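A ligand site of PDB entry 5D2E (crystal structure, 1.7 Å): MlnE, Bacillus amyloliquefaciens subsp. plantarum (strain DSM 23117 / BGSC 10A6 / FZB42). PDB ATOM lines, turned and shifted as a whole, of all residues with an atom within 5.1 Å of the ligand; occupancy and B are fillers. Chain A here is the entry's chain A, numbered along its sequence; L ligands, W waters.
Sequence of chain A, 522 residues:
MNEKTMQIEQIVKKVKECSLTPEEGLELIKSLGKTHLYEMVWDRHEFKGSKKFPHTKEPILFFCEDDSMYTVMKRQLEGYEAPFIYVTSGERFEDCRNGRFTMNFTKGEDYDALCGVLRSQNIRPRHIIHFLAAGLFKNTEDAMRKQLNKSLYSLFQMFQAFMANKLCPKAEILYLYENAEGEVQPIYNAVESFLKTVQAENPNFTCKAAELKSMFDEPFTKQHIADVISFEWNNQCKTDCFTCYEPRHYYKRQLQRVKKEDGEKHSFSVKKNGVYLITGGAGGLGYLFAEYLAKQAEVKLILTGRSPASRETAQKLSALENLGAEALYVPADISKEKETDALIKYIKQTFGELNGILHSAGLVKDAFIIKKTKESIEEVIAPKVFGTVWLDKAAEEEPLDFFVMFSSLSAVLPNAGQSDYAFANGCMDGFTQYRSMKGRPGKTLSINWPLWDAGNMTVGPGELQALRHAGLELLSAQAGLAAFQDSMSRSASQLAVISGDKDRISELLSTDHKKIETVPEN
Water W5 bridges an oxygen (O13) of the ligand (2.6 Å) and the backbone NH (N) of Leu 363 (3.3 Å). Water W1 bridges the side-chain hydroxyl of Tyr 329 and an oxygen (O16) of the ligand. Water W6 lies within hydrogen-bond range of an oxygen (O9) of the ligand (2.8 Å), the backbone NH (N) of Gly 286 (2.9 Å), the side-chain hydroxyl (OG) of Ser 360 (2.9 Å) and the backbone carbonyl oxygen (O) of Gly 280 (2.9 Å). Water W9 bridges the backbone carbonyl oxygen (O) of Gly 362 (2.6 Å) and an oxygen (O2) of the ligand (2.8 Å). Water W3 lies within hydrogen-bond range of the backbone NH (N) of Ala 282 (2.9 Å), an oxygen (O5) of the ligand (2.9 Å), the backbone NH (N) of Gly 283 (3.3 Å) and the backbone carbonyl oxygen (O) of Gly 280 (3.5 Å). Water W4 lies within hydrogen-bond range of O of Ala 361 (2.7 Å), NZ of Lys 384 (2.8 Å) and O12 of the ligand (3.4 Å).
The backbone carbonyl oxygen of Ala 332 sits close to a nitrogen (N4) of the ligand (3.4 Å). CA of Gly 280 touches O4 of the ligand, at 3.6 Å. Gly 305 touches the ligand. Leu 363 touches the ligand. Phe 406 touches the ligand (CB to O11, 3.8 Å). Ser 407 touches the ligand (O to C21, 3.2 Å). CB of Ser 408 touches C21 of the ligand, at 3.9 Å. O of Trp 449 touches C20 of the ligand (3.3 Å). Pro 450 touches the ligand (O to C19, 3.0 Å). Leu 451 touches the ligand (CA to O14, 3.3 Å). 23 residues have an atom within 4 Å of the ligand: Gly 280, Gly 283, Gly 284, Leu 285, Gly 305, Arg 306, Ser 307, Ala 332, Asp 333, Ile 334, Ser 360, Ala 361, Gly 362, Leu 363, Lys 384, Phe 406, Ser 407, Ser 408, Tyr 421, Trp 449, Pro 450, Leu 451 and Trp 452.
The side-chain hydroxyl (OH) of Tyr 421 sits at hydrogen-bond distance from an oxygen (O13) of the ligand (2.4 Å). An oxygen (O16) of the ligand lies within hydrogen-bond range of the backbone NH of Ser 307, 2.9 Å away. The side-chain hydroxyl (OG) of Ser 307 lies within hydrogen-bond range of an oxygen (O16) of the ligand. N of Arg 306 lies within hydrogen-bond range of O17 of the ligand (2.7 Å). An oxygen (O17) of the ligand is in salt-bridge range of the guanidinium group (NE) of Arg 306, 2.9 Å away. The side-chain amino group (NZ) of Lys 384 sits at hydrogen-bond distance from an oxygen (O12) of the ligand (2.7 Å). The backbone NH (N) of Leu 285 is in hydrogen-bond range of an oxygen (O9) of the ligand, at 2.8 Å. N of Gly 284 lies within hydrogen-bond range of O1 of the ligand. O of Ser 360 is in hydrogen-bond range of O12 of the ligand, at 2.9 Å. The backbone NH (N) of Trp 452 sits at hydrogen-bond distance from an oxygen (O14) of the ligand (2.9 Å). The side-chain carboxylate of Asp 333 sits at hydrogen-bond distance from a nitrogen (N3) of the ligand. N of Ile 334 sits at hydrogen-bond distance from N4 of the ligand (3.1 Å). An oxygen (O4) of the ligand is in hydrogen-bond range of the backbone NH (N) of Gly 362, at 3.2 Å. O of Ala 361 is in hydrogen-bond range of O12 of the ligand (3.3 Å). The backbone NH (N) of Gly 283 sits close to an oxygen (O5) of the ligand, at 3.5 Å.
The backbone carbonyl oxygen of Tyr 421 lies within hydrogen-bond range of the side-chain amide nitrogen of Asn 425 (2.9 Å). O of Ser 307 lies within hydrogen-bond range of OH of Tyr 329 (2.7 Å). The side-chain carboxylate of Asp 333 sits at hydrogen-bond distance from the side-chain hydroxyl of Ser 335. The backbone carbonyl oxygen (O) of Ser 407 is in hydrogen-bond range of the backbone NH (N) of Trp 449 (3.2 Å). O of Asn 425 lies within hydrogen-bond range of OG of Ser 407 (3.2 Å). The backbone carbonyl oxygen (O) of Gly 305 lies within hydrogen-bond range of the backbone NH (N) of Ala 332, at 2.8 Å. O of Gly 305 lies within hydrogen-bond range of OH of Tyr 329, at 3.4 Å. The backbone carbonyl oxygen (O) of Thr 304 lies within hydrogen-bond range of the backbone NH (N) of Gly 280 (2.7 Å).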
ATOM      1  N   GLY A 280     -21.063  25.559 -30.717  1.00  0.00           N
ATOM      2  CA  GLY A 280     -20.791  24.156 -31.097  1.00  0.00           C
ATOM      3  C   GLY A 280     -21.922  23.224 -30.684  1.00  0.00           C
ATOM      4  O   GLY A 280     -21.713  22.027 -30.433  1.00  0.00           O
ATOM      5  N   ALA A 282     -24.418  21.850 -32.254  1.00  0.00           N
ATOM      6  CA  ALA A 282     -24.714  20.645 -33.046  1.00  0.00           C
ATOM      7  C   ALA A 282     -23.584  19.581 -32.992  1.00  0.00           C
ATOM      8  O   ALA A 282     -23.753  18.514 -33.550  1.00  0.00           O
ATOM      9  CB  ALA A 282     -25.016  21.020 -34.476  1.00  0.00           C
ATOM     10  N   GLY A 283     -22.436  19.900 -32.382  1.00  0.00           N
ATOM     11  CA  GLY A 283     -21.299  18.974 -32.240  1.00  0.00           C
ATOM     12  C   GLY A 283     -21.575  17.960 -31.118  1.00  0.00           C
ATOM     13  O   GLY A 283     -22.612  17.937 -30.546  1.00  0.00           O
ATOM     14  N   GLY A 284     -20.632  17.092 -30.875  1.00  0.00           N
ATOM     15  CA  GLY A 284     -20.801  15.991 -29.952  1.00  0.00           C
ATOM     16  C   GLY A 284     -21.162  16.406 -28.533  1.00  0.00           C
ATOM     17  O   GLY A 284     -22.264  16.094 -28.059  1.00  0.00           O
ATOM     18  N   LEU A 285     -20.270  17.108 -27.855  1.00  0.00           N
ATOM     19  CA  LEU A 285     -20.568  17.513 -26.473  1.00  0.00           C
ATOM     20  C   LEU A 285     -21.653  18.530 -26.425  1.00  0.00           C
ATOM     21  O   LEU A 285     -22.538  18.504 -25.545  1.00  0.00           O
ATOM     22  CB  LEU A 285     -19.314  18.073 -25.800  1.00  0.00           C
ATOM     23  CG  LEU A 285     -18.210  17.071 -25.525  1.00  0.00           C
ATOM     24  CD1 LEU A 285     -17.213  17.624 -24.513  1.00  0.00           C
ATOM     25  CD2 LEU A 285     -18.807  15.738 -25.043  1.00  0.00           C
ATOM     26  N   GLY A 286     -21.611  19.464 -27.348  1.00  0.00           N
ATOM     27  CA  GLY A 286     -22.631  20.555 -27.404  1.00  0.00           C
ATOM     28  C   GLY A 286     -24.078  20.007 -27.403  1.00  0.00           C
ATOM     29  O   GLY A 286     -24.969  20.511 -26.691  1.00  0.00           O
ATOM     30  N   THR A 304     -25.464  26.884 -31.947  1.00  0.00           N
ATOM     31  CA  THR A 304     -24.742  27.643 -32.940  1.00  0.00           C
ATOM     32  C   THR A 304     -23.533  26.866 -33.379  1.00  0.00           C
ATOM     33  O   THR A 304     -22.860  26.194 -32.589  1.00  0.00           O
ATOM     34  CB  THR A 304     -24.396  29.075 -32.468  1.00  0.00           C
ATOM     35  OG1 THR A 304     -25.594  29.745 -32.108  1.00  0.00           O
ATOM     36  CG2 THR A 304     -23.845  29.834 -33.545  1.00  0.00           C
ATOM     37  N   GLY A 305     -23.328  26.866 -34.687  1.00  0.00           N
ATOM     38  CA  GLY A 305     -22.080  26.371 -35.330  1.00  0.00           C
ATOM     39  C   GLY A 305     -21.917  27.177 -36.620  1.00  0.00           C
ATOM     40  O   GLY A 305     -22.789  27.964 -37.002  1.00  0.00           O
ATOM     41  N   ARG A 306     -20.791  27.015 -37.296  1.00  0.00           N
ATOM     42  CA  ARG A 306     -20.536  27.776 -38.510  1.00  0.00           C
ATOM     43  C   ARG A 306     -21.350  27.241 -39.701  1.00  0.00           C
ATOM     44  O   ARG A 306     -21.782  28.026 -40.528  1.00  0.00           O
ATOM     45  CB  ARG A 306     -19.062  27.687 -38.868  1.00  0.00           C
ATOM     46  CG  ARG A 306     -18.221  28.632 -37.996  1.00  0.00           C
ATOM     47  CD  ARG A 306     -16.780  28.338 -38.212  1.00  0.00           C
ATOM     48  NE  ARG A 306     -16.553  26.924 -37.932  1.00  0.00           N
ATOM     49  CZ  ARG A 306     -15.442  26.280 -38.252  1.00  0.00           C
ATOM     50  NH1 ARG A 306     -14.440  26.969 -38.801  1.00  0.00           N
ATOM     51  NH2 ARG A 306     -15.308  24.983 -37.954  1.00  0.00           N
ATOM     52  N   SER A 307     -21.533  25.919 -39.729  1.00  0.00           N
ATOM     53  CA  SER A 307     -22.147  25.251 -40.882  1.00  0.00           C
ATOM     54  C   SER A 307     -23.605  25.653 -41.102  1.00  0.00           C
ATOM     55  O   SER A 307     -24.367  25.867 -40.145  1.00  0.00           O
ATOM     56  CB  SER A 307     -22.141  23.757 -40.687  1.00  0.00           C
ATOM     57  OG  SER A 307     -20.830  23.318 -40.575  1.00  0.00           O
ATOM     58  N   TYR A 329     -31.460  26.437 -34.491  1.00  0.00           N
ATOM     59  CA  TYR A 329     -30.073  26.345 -34.965  1.00  0.00           C
ATOM     60  C   TYR A 329     -29.780  27.609 -35.701  1.00  0.00           C
ATOM     61  O   TYR A 329     -30.349  27.889 -36.731  1.00  0.00           O
ATOM     62  CB  TYR A 329     -29.809  25.148 -35.844  1.00  0.00           C
ATOM     63  CG  TYR A 329     -28.381  25.091 -36.342  1.00  0.00           C
ATOM     64  CD1 TYR A 329     -27.343  24.726 -35.463  1.00  0.00           C
ATOM     65  CD2 TYR A 329     -28.043  25.446 -37.652  1.00  0.00           C
ATOM     66  CE1 TYR A 329     -25.992  24.727 -35.905  1.00  0.00           C
ATOM     67  CE2 TYR A 329     -26.704  25.435 -38.089  1.00  0.00           C
ATOM     68  CZ  TYR A 329     -25.678  25.053 -37.217  1.00  0.00           C
ATOM     69  OH  TYR A 329     -24.345  25.043 -37.592  1.00  0.00           O
ATOM     70  N   ALA A 332     -23.362  30.721 -37.196  1.00  0.00           N
ATOM     71  CA  ALA A 332     -22.544  31.895 -36.894  1.00  0.00           C
ATOM     72  C   ALA A 332     -21.120  31.432 -36.639  1.00  0.00           C
ATOM     73  O   ALA A 332     -20.893  30.320 -36.133  1.00  0.00           O
ATOM     74  CB  ALA A 332     -23.065  32.663 -35.706  1.00  0.00           C
ATOM     75  N   ASP A 333     -20.176  32.256 -37.035  1.00  0.00           N
ATOM     76  CA  ASP A 333     -18.775  32.002 -36.743  1.00  0.00           C
ATOM     77  C   ASP A 333     -18.470  32.888 -35.511  1.00  0.00           C
ATOM     78  O   ASP A 333     -18.286  34.078 -35.620  1.00  0.00           O
ATOM     79  CB  ASP A 333     -17.906  32.331 -37.933  1.00  0.00           C
ATOM     80  CG  ASP A 333     -16.461  32.101 -37.662  1.00  0.00           C
ATOM     81  OD1 ASP A 333     -16.118  31.973 -36.468  1.00  0.00           O
ATOM     82  OD2 ASP A 333     -15.680  32.104 -38.641  1.00  0.00           O
ATOM     83  N   ILE A 334     -18.501  32.293 -34.332  1.00  0.00           N
ATOM     84  CA  ILE A 334     -18.401  33.124 -33.135  1.00  0.00           C
ATOM     85  C   ILE A 334     -17.012  33.703 -32.884  1.00  0.00           C
ATOM     86  O   ILE A 334     -16.881  34.498 -31.988  1.00  0.00           O
ATOM     87  CB  ILE A 334     -18.987  32.488 -31.870  1.00  0.00           C
ATOM     88  CG1 ILE A 334     -18.548  31.097 -31.611  1.00  0.00           C
ATOM     89  CG2 ILE A 334     -20.527  32.402 -31.928  1.00  0.00           C
ATOM     90  CD1 ILE A 334     -17.105  30.950 -31.382  1.00  0.00           C
ATOM     91  N   SER A 335     -16.004  33.346 -33.695  1.00  0.00           N
ATOM     92  CA  SER A 335     -14.694  34.036 -33.693  1.00  0.00           C
ATOM     93  C   SER A 335     -14.732  35.398 -34.361  1.00  0.00           C
ATOM     94  O   SER A 335     -13.724  36.142 -34.365  1.00  0.00           O
ATOM     95  CB  SER A 335     -13.653  33.155 -34.394  1.00  0.00           C
ATOM     96  OG  SER A 335     -13.794  33.246 -35.806  1.00  0.00           O
ATOM     97  N   SER A 360     -18.900  25.517 -26.381  1.00  0.00           N
ATOM     98  CA  SER A 360     -18.356  24.192 -26.738  1.00  0.00           C
ATOM     99  C   SER A 360     -17.712  24.244 -28.115  1.00  0.00           C
ATOM    100  O   SER A 360     -17.127  23.243 -28.549  1.00  0.00           O
ATOM    101  CB  SER A 360     -19.485  23.126 -26.769  1.00  0.00           C
ATOM    102  OG  SER A 360     -18.952  21.844 -26.768  1.00  0.00           O
ATOM    103  N   ALA A 361     -17.814  25.367 -28.809  1.00  0.00           N
ATOM    104  CA  ALA A 361     -17.209  25.515 -30.116  1.00  0.00           C
ATOM    105  C   ALA A 361     -15.705  25.290 -30.034  1.00  0.00           C
ATOM    106  O   ALA A 361     -15.010  25.738 -29.093  1.00  0.00           O
ATOM    107  CB  ALA A 361     -17.470  26.912 -30.664  1.00  0.00           C
ATOM    108  N   GLY A 362     -15.197  24.564 -31.001  1.00  0.00           N
ATOM    109  CA  GLY A 362     -13.788  24.249 -31.053  1.00  0.00           C
ATOM    110  C   GLY A 362     -13.422  23.361 -32.221  1.00  0.00           C
ATOM    111  O   GLY A 362     -14.295  22.814 -32.912  1.00  0.00           O
ATOM    112  N   LEU A 363     -12.126  23.345 -32.507  1.00  0.00           N
ATOM    113  CA  LEU A 363     -11.599  22.387 -33.454  1.00  0.00           C
ATOM    114  C   LEU A 363     -10.218  21.954 -33.095  1.00  0.00           C
ATOM    115  O   LEU A 363      -9.524  22.605 -32.338  1.00  0.00           O
ATOM    116  CB  LEU A 363     -11.613  22.916 -34.849  1.00  0.00           C
ATOM    117  CG  LEU A 363     -10.966  24.204 -35.146  1.00  0.00           C
ATOM    118  CD1 LEU A 363     -10.095  24.045 -36.393  1.00  0.00           C
ATOM    119  CD2 LEU A 363     -12.050  25.219 -35.459  1.00  0.00           C
ATOM    120  N   PRO A 383     -11.861  29.962 -32.158  1.00  0.00           N
ATOM    121  CA  PRO A 383     -13.095  29.942 -31.369  1.00  0.00           C
ATOM    122  C   PRO A 383     -12.951  30.079 -29.861  1.00  0.00           C
ATOM    123  O   PRO A 383     -13.889  30.519 -29.165  1.00  0.00           O
ATOM    124  CB  PRO A 383     -13.696  28.583 -31.689  1.00  0.00           C
ATOM    125  CG  PRO A 383     -12.543  27.734 -32.163  1.00  0.00           C
ATOM    126  CD  PRO A 383     -11.609  28.678 -32.831  1.00  0.00           C
ATOM    127  N   LYS A 384     -11.802  29.636 -29.354  1.00  0.00           N
ATOM    128  CA  LYS A 384     -11.535  29.540 -27.924  1.00  0.00           C
ATOM    129  C   LYS A 384     -10.804  30.796 -27.391  1.00  0.00           C
ATOM    130  O   LYS A 384     -10.882  31.113 -26.230  1.00  0.00           O
ATOM    131  CB  LYS A 384     -10.734  28.270 -27.651  1.00  0.00           C
ATOM    132  CG  LYS A 384     -11.571  27.006 -27.698  1.00  0.00           C
ATOM    133  CD  LYS A 384     -10.782  25.782 -27.659  1.00  0.00           C
ATOM    134  CE  LYS A 384     -11.656  24.523 -27.753  1.00  0.00           C
ATOM    135  NZ  LYS A 384     -12.478  24.334 -26.547  1.00  0.00           N
ATOM    136  N   PHE A 406     -15.941  25.025 -22.206  1.00  0.00           N
ATOM    137  CA  PHE A 406     -15.506  23.595 -22.345  1.00  0.00           C
ATOM    138  C   PHE A 406     -14.054  23.572 -22.774  1.00  0.00           C
ATOM    139  O   PHE A 406     -13.708  23.677 -23.965  1.00  0.00           O
ATOM    140  CB  PHE A 406     -16.416  22.864 -23.356  1.00  0.00           C
ATOM    141  CG  PHE A 406     -17.793  22.465 -22.785  1.00  0.00           C
ATOM    142  CD1 PHE A 406     -18.250  22.888 -21.533  1.00  0.00           C
ATOM    143  CD2 PHE A 406     -18.630  21.650 -23.504  1.00  0.00           C
ATOM    144  CE1 PHE A 406     -19.450  22.488 -20.994  1.00  0.00           C
ATOM    145  CE2 PHE A 406     -19.869  21.258 -22.974  1.00  0.00           C
ATOM    146  CZ  PHE A 406     -20.272  21.661 -21.724  1.00  0.00           C
ATOM    147  N   SER A 407     -13.197  23.514 -21.760  1.00  0.00           N
ATOM    148  CA  SER A 407     -11.786  23.526 -21.965  1.00  0.00           C
ATOM    149  C   SER A 407     -11.305  22.060 -22.030  1.00  0.00           C
ATOM    150  O   SER A 407     -12.102  21.139 -22.185  1.00  0.00           O
ATOM    151  CB  SER A 407     -11.136  24.360 -20.836  1.00  0.00           C
ATOM    152  OG  SER A 407      -9.755  24.552 -21.099  1.00  0.00           O
ATOM    153  N   SER A 408     -10.000  21.850 -21.951  1.00  0.00           N
ATOM    154  CA  SER A 408      -9.416  20.578 -22.149  1.00  0.00           C
ATOM    155  C   SER A 408      -8.330  20.384 -21.151  1.00  0.00           C
ATOM    156  O   SER A 408      -7.586  21.303 -20.801  1.00  0.00           O
ATOM    157  CB  SER A 408      -8.858  20.498 -23.603  1.00  0.00           C
ATOM    158  OG  SER A 408      -8.026  19.363 -23.757  1.00  0.00           O
ATOM    159  N   TYR A 421      -3.796  24.046 -29.551  1.00  0.00           N
ATOM    160  CA  TYR A 421      -5.052  23.618 -28.882  1.00  0.00           C
ATOM    161  C   TYR A 421      -4.939  23.773 -27.364  1.00  0.00           C
ATOM    162  O   TYR A 421      -5.867  24.276 -26.711  1.00  0.00           O
ATOM    163  CB  TYR A 421      -5.382  22.168 -29.270  1.00  0.00           C
ATOM    164  CG  TYR A 421      -6.675  21.601 -28.756  1.00  0.00           C
ATOM    165  CD1 TYR A 421      -7.909  21.975 -29.299  1.00  0.00           C
ATOM    166  CD2 TYR A 421      -6.662  20.620 -27.764  1.00  0.00           C
ATOM    167  CE1 TYR A 421      -9.097  21.443 -28.820  1.00  0.00           C
ATOM    168  CE2 TYR A 421      -7.856  20.069 -27.300  1.00  0.00           C
ATOM    169  CZ  TYR A 421      -9.052  20.480 -27.829  1.00  0.00           C
ATOM    170  OH  TYR A 421     -10.180  19.910 -27.346  1.00  0.00           O
ATOM    171  N   ASN A 425      -7.206  26.464 -25.060  1.00  0.00           N
ATOM    172  CA  ASN A 425      -7.992  26.069 -23.947  1.00  0.00           C
ATOM    173  C   ASN A 425      -7.482  26.785 -22.693  1.00  0.00           C
ATOM    174  O   ASN A 425      -8.265  27.256 -21.881  1.00  0.00           O
ATOM    175  CB  ASN A 425      -7.991  24.563 -23.808  1.00  0.00           C
ATOM    176  CG  ASN A 425      -8.955  23.914 -24.827  1.00  0.00           C
ATOM    177  OD1 ASN A 425     -10.165  24.069 -24.720  1.00  0.00           O
ATOM    178  ND2 ASN A 425      -8.410  23.282 -25.859  1.00  0.00           N
ATOM    179  N   TRP A 449     -11.953  19.309 -19.539  1.00  0.00           N
ATOM    180  CA  TRP A 449     -12.410  17.951 -19.867  1.00  0.00           C
ATOM    181  C   TRP A 449     -11.301  17.020 -20.405  1.00  0.00           C
ATOM    182  O   TRP A 449     -10.476  17.444 -21.195  1.00  0.00           O
ATOM    183  CB  TRP A 449     -13.441  18.023 -20.955  1.00  0.00           C
ATOM    184  CG  TRP A 449     -14.716  18.664 -20.617  1.00  0.00           C
ATOM    185  CD1 TRP A 449     -15.264  19.763 -21.254  1.00  0.00           C
ATOM    186  CD2 TRP A 449     -15.674  18.276 -19.628  1.00  0.00           C
ATOM    187  NE1 TRP A 449     -16.452  20.061 -20.724  1.00  0.00           N
ATOM    188  CE2 TRP A 449     -16.747  19.172 -19.722  1.00  0.00           C
ATOM    189  CE3 TRP A 449     -15.737  17.246 -18.679  1.00  0.00           C
ATOM    190  CZ2 TRP A 449     -17.914  19.056 -18.912  1.00  0.00           C
ATOM    191  CZ3 TRP A 449     -16.939  17.096 -17.907  1.00  0.00           C
ATOM    192  CH2 TRP A 449     -17.972  18.051 -17.990  1.00  0.00           C
ATOM    193  N   PRO A 450     -11.296  15.766 -19.973  1.00  0.00           N
ATOM    194  CA  PRO A 450     -10.505  14.755 -20.614  1.00  0.00           C
ATOM    195  C   PRO A 450     -11.258  14.220 -21.845  1.00  0.00           C
ATOM    196  O   PRO A 450     -12.314  14.761 -22.222  1.00  0.00           O
ATOM    197  CB  PRO A 450     -10.392  13.707 -19.521  1.00  0.00           C
ATOM    198  CG  PRO A 450     -11.788  13.710 -18.987  1.00  0.00           C
ATOM    199  CD  PRO A 450     -12.287  15.147 -19.093  1.00  0.00           C
ATOM    200  N   LEU A 451     -10.688  13.186 -22.487  1.00  0.00           N
ATOM    201  CA  LEU A 451     -11.360  12.516 -23.637  1.00  0.00           C
ATOM    202  C   LEU A 451     -12.615  11.791 -23.181  1.00  0.00           C
ATOM    203  O   LEU A 451     -12.625  11.095 -22.153  1.00  0.00           O
ATOM    204  CB  LEU A 451     -10.461  11.485 -24.313  1.00  0.00           C
ATOM    205  CG  LEU A 451      -9.462  12.114 -25.229  1.00  0.00           C
ATOM    206  CD1 LEU A 451      -8.456  11.040 -25.670  1.00  0.00           C
ATOM    207  CD2 LEU A 451     -10.197  12.759 -26.403  1.00  0.00           C
ATOM    208  N   TRP A 452     -13.679  12.072 -23.894  1.00  0.00           N
ATOM    209  CA  TRP A 452     -14.964  11.471 -23.635  1.00  0.00           C
ATOM    210  C   TRP A 452     -15.196  10.284 -24.614  1.00  0.00           C
ATOM    211  O   TRP A 452     -14.677  10.282 -25.716  1.00  0.00           O
ATOM    212  CB  TRP A 452     -16.083  12.383 -23.933  1.00  0.00           C
ATOM    213  CG  TRP A 452     -16.288  13.542 -23.048  1.00  0.00           C
ATOM    214  CD1 TRP A 452     -15.409  14.556 -22.852  1.00  0.00           C
ATOM    215  CD2 TRP A 452     -17.465  13.860 -22.312  1.00  0.00           C
ATOM    216  NE1 TRP A 452     -15.964  15.478 -22.003  1.00  0.00           N
ATOM    217  CE2 TRP A 452     -17.242  15.102 -21.684  1.00  0.00           C
ATOM    218  CE3 TRP A 452     -18.714  13.229 -22.149  1.00  0.00           C
ATOM    219  CZ2 TRP A 452     -18.201  15.710 -20.889  1.00  0.00           C
ATOM    220  CZ3 TRP A 452     -19.668  13.845 -21.365  1.00  0.00           C
ATOM    221  CH2 TRP A 452     -19.415  15.084 -20.738  1.00  0.00           C
ATOM    222  N   ALA A 454     -18.143   9.656 -26.165  1.00  0.00           N
ATOM    223  CA  ALA A 454     -19.432  10.301 -26.549  1.00  0.00           C
ATOM    224  C   ALA A 454     -19.199  11.378 -27.626  1.00  0.00           C
ATOM    225  O   ALA A 454     -18.130  11.998 -27.674  1.00  0.00           O
ATOM    226  CB  ALA A 454     -20.153  10.913 -25.346  1.00  0.00           C
HETATM  227  P1  LIG L   1     -17.135  18.673 -32.139  1.00  0.00           P
HETATM  228  O1  LIG L   1     -18.240  17.596 -32.266  1.00  0.00           O
HETATM  229  O2  LIG L   1     -16.222  19.063 -33.288  1.00  0.00           O
HETATM  230  O3  LIG L   1     -17.975  19.993 -31.771  1.00  0.00           O
HETATM  231  C1  LIG L   1     -17.322  21.260 -31.792  1.00  0.00           C
HETATM  232  C2  LIG L   1     -18.260  22.131 -32.581  1.00  0.00           C
HETATM  233  O4  LIG L   1     -17.676  23.448 -32.657  1.00  0.00           O
HETATM  234  C3  LIG L   1     -18.484  21.685 -34.063  1.00  0.00           C
HETATM  235  O5  LIG L   1     -19.833  21.242 -34.250  1.00  0.00           O
HETATM  236  C4  LIG L   1     -18.234  22.960 -34.879  1.00  0.00           C
HETATM  237  O6  LIG L   1     -19.219  23.130 -35.863  1.00  0.00           O
HETATM  238  C5  LIG L   1     -18.240  24.062 -33.796  1.00  0.00           C
HETATM  239  N1  LIG L   1     -17.400  25.217 -34.103  1.00  0.00           N
HETATM  240  C6  LIG L   1     -16.048  25.229 -34.410  1.00  0.00           C
HETATM  241  N2  LIG L   1     -15.617  26.505 -34.707  1.00  0.00           N
HETATM  242  C7  LIG L   1     -16.675  27.314 -34.504  1.00  0.00           C
HETATM  243  C8  LIG L   1     -16.924  28.734 -34.617  1.00  0.00           C
HETATM  244  N3  LIG L   1     -15.868  29.541 -34.965  1.00  0.00           N
HETATM  245  N4  LIG L   1     -18.234  29.202 -34.412  1.00  0.00           N
HETATM  246  C9  LIG L   1     -19.219  28.355 -34.074  1.00  0.00           C
HETATM  247  N5  LIG L   1     -19.055  27.009 -33.942  1.00  0.00           N
HETATM  248  C10 LIG L   1     -17.852  26.459 -34.145  1.00  0.00           C
HETATM  249  O7  LIG L   1     -16.176  18.362 -30.856  1.00  0.00           O
HETATM  250  P2  LIG L   1     -16.655  17.796 -29.404  1.00  0.00           P
HETATM  251  O8  LIG L   1     -16.007  16.448 -29.144  1.00  0.00           O
HETATM  252  O9  LIG L   1     -18.119  18.130 -29.296  1.00  0.00           O
HETATM  253  O10 LIG L   1     -15.960  18.779 -28.318  1.00  0.00           O
HETATM  254  C11 LIG L   1     -16.672  20.018 -28.038  1.00  0.00           C
HETATM  255  C12 LIG L   1     -15.858  20.943 -27.118  1.00  0.00           C
HETATM  256  O11 LIG L   1     -15.390  20.278 -25.960  1.00  0.00           O
HETATM  257  C13 LIG L   1     -14.618  21.434 -27.866  1.00  0.00           C
HETATM  258  O12 LIG L   1     -14.457  22.825 -27.628  1.00  0.00           O
HETATM  259  C14 LIG L   1     -13.468  20.610 -27.315  1.00  0.00           C
HETATM  260  O13 LIG L   1     -12.186  21.296 -27.418  1.00  0.00           O
HETATM  261  C15 LIG L   1     -13.934  20.268 -25.865  1.00  0.00           C
HETATM  262  N6  LIG L   1     -13.339  18.976 -25.434  1.00  0.00           N
HETATM  263  C16 LIG L   1     -13.792  17.771 -25.934  1.00  0.00           C
HETATM  264  C17 LIG L   1     -13.267  16.522 -25.570  1.00  0.00           C
HETATM  265  C18 LIG L   1     -13.813  15.187 -26.141  1.00  0.00           C
HETATM  266  O14 LIG L   1     -13.273  14.112 -25.851  1.00  0.00           O
HETATM  267  N7  LIG L   1     -14.883  15.110 -26.941  1.00  0.00           N
HETATM  268  C19 LIG L   1     -12.182  16.519 -24.676  1.00  0.00           C
HETATM  269  C20 LIG L   1     -11.693  17.745 -24.202  1.00  0.00           C
HETATM  270  C21 LIG L   1     -12.293  18.961 -24.571  1.00  0.00           C
HETATM  271  P3  LIG L   1     -19.000  23.990 -37.248  1.00  0.00           P
HETATM  272  O15 LIG L   1     -17.826  23.412 -38.021  1.00  0.00           O
HETATM  273  O16 LIG L   1     -20.373  23.904 -37.990  1.00  0.00           O
HETATM  274  O17 LIG L   1     -18.694  25.394 -36.793  1.00  0.00           O
HETATM  275  O   HOH W   1     -22.742  23.177 -36.752  1.00  0.00           O
HETATM  276  O   HOH W   2     -17.373  24.289 -40.638  1.00  0.00           O
HETATM  277  O   HOH W   3     -22.204  22.862 -33.786  1.00  0.00           O
HETATM  278  O   HOH W   4     -14.748  25.974 -26.428  1.00  0.00           O
HETATM  279  O   HOH W   5     -12.603  21.356 -29.938  1.00  0.00           O
HETATM  280  O   HOH W   6     -19.651  20.446 -29.177  1.00  0.00           O
HETATM  281  O   HOH W   7     -13.489  28.106 -35.522  1.00  0.00           O
HETATM  282  O   HOH W   8      -9.049  17.003 -25.162  1.00  0.00           O
HETATM  283  O   HOH W   9     -14.915  21.101 -34.779  1.00  0.00           O
HETATM  284  O   HOH W  10     -20.093  19.661 -36.376  1.00  0.00           O
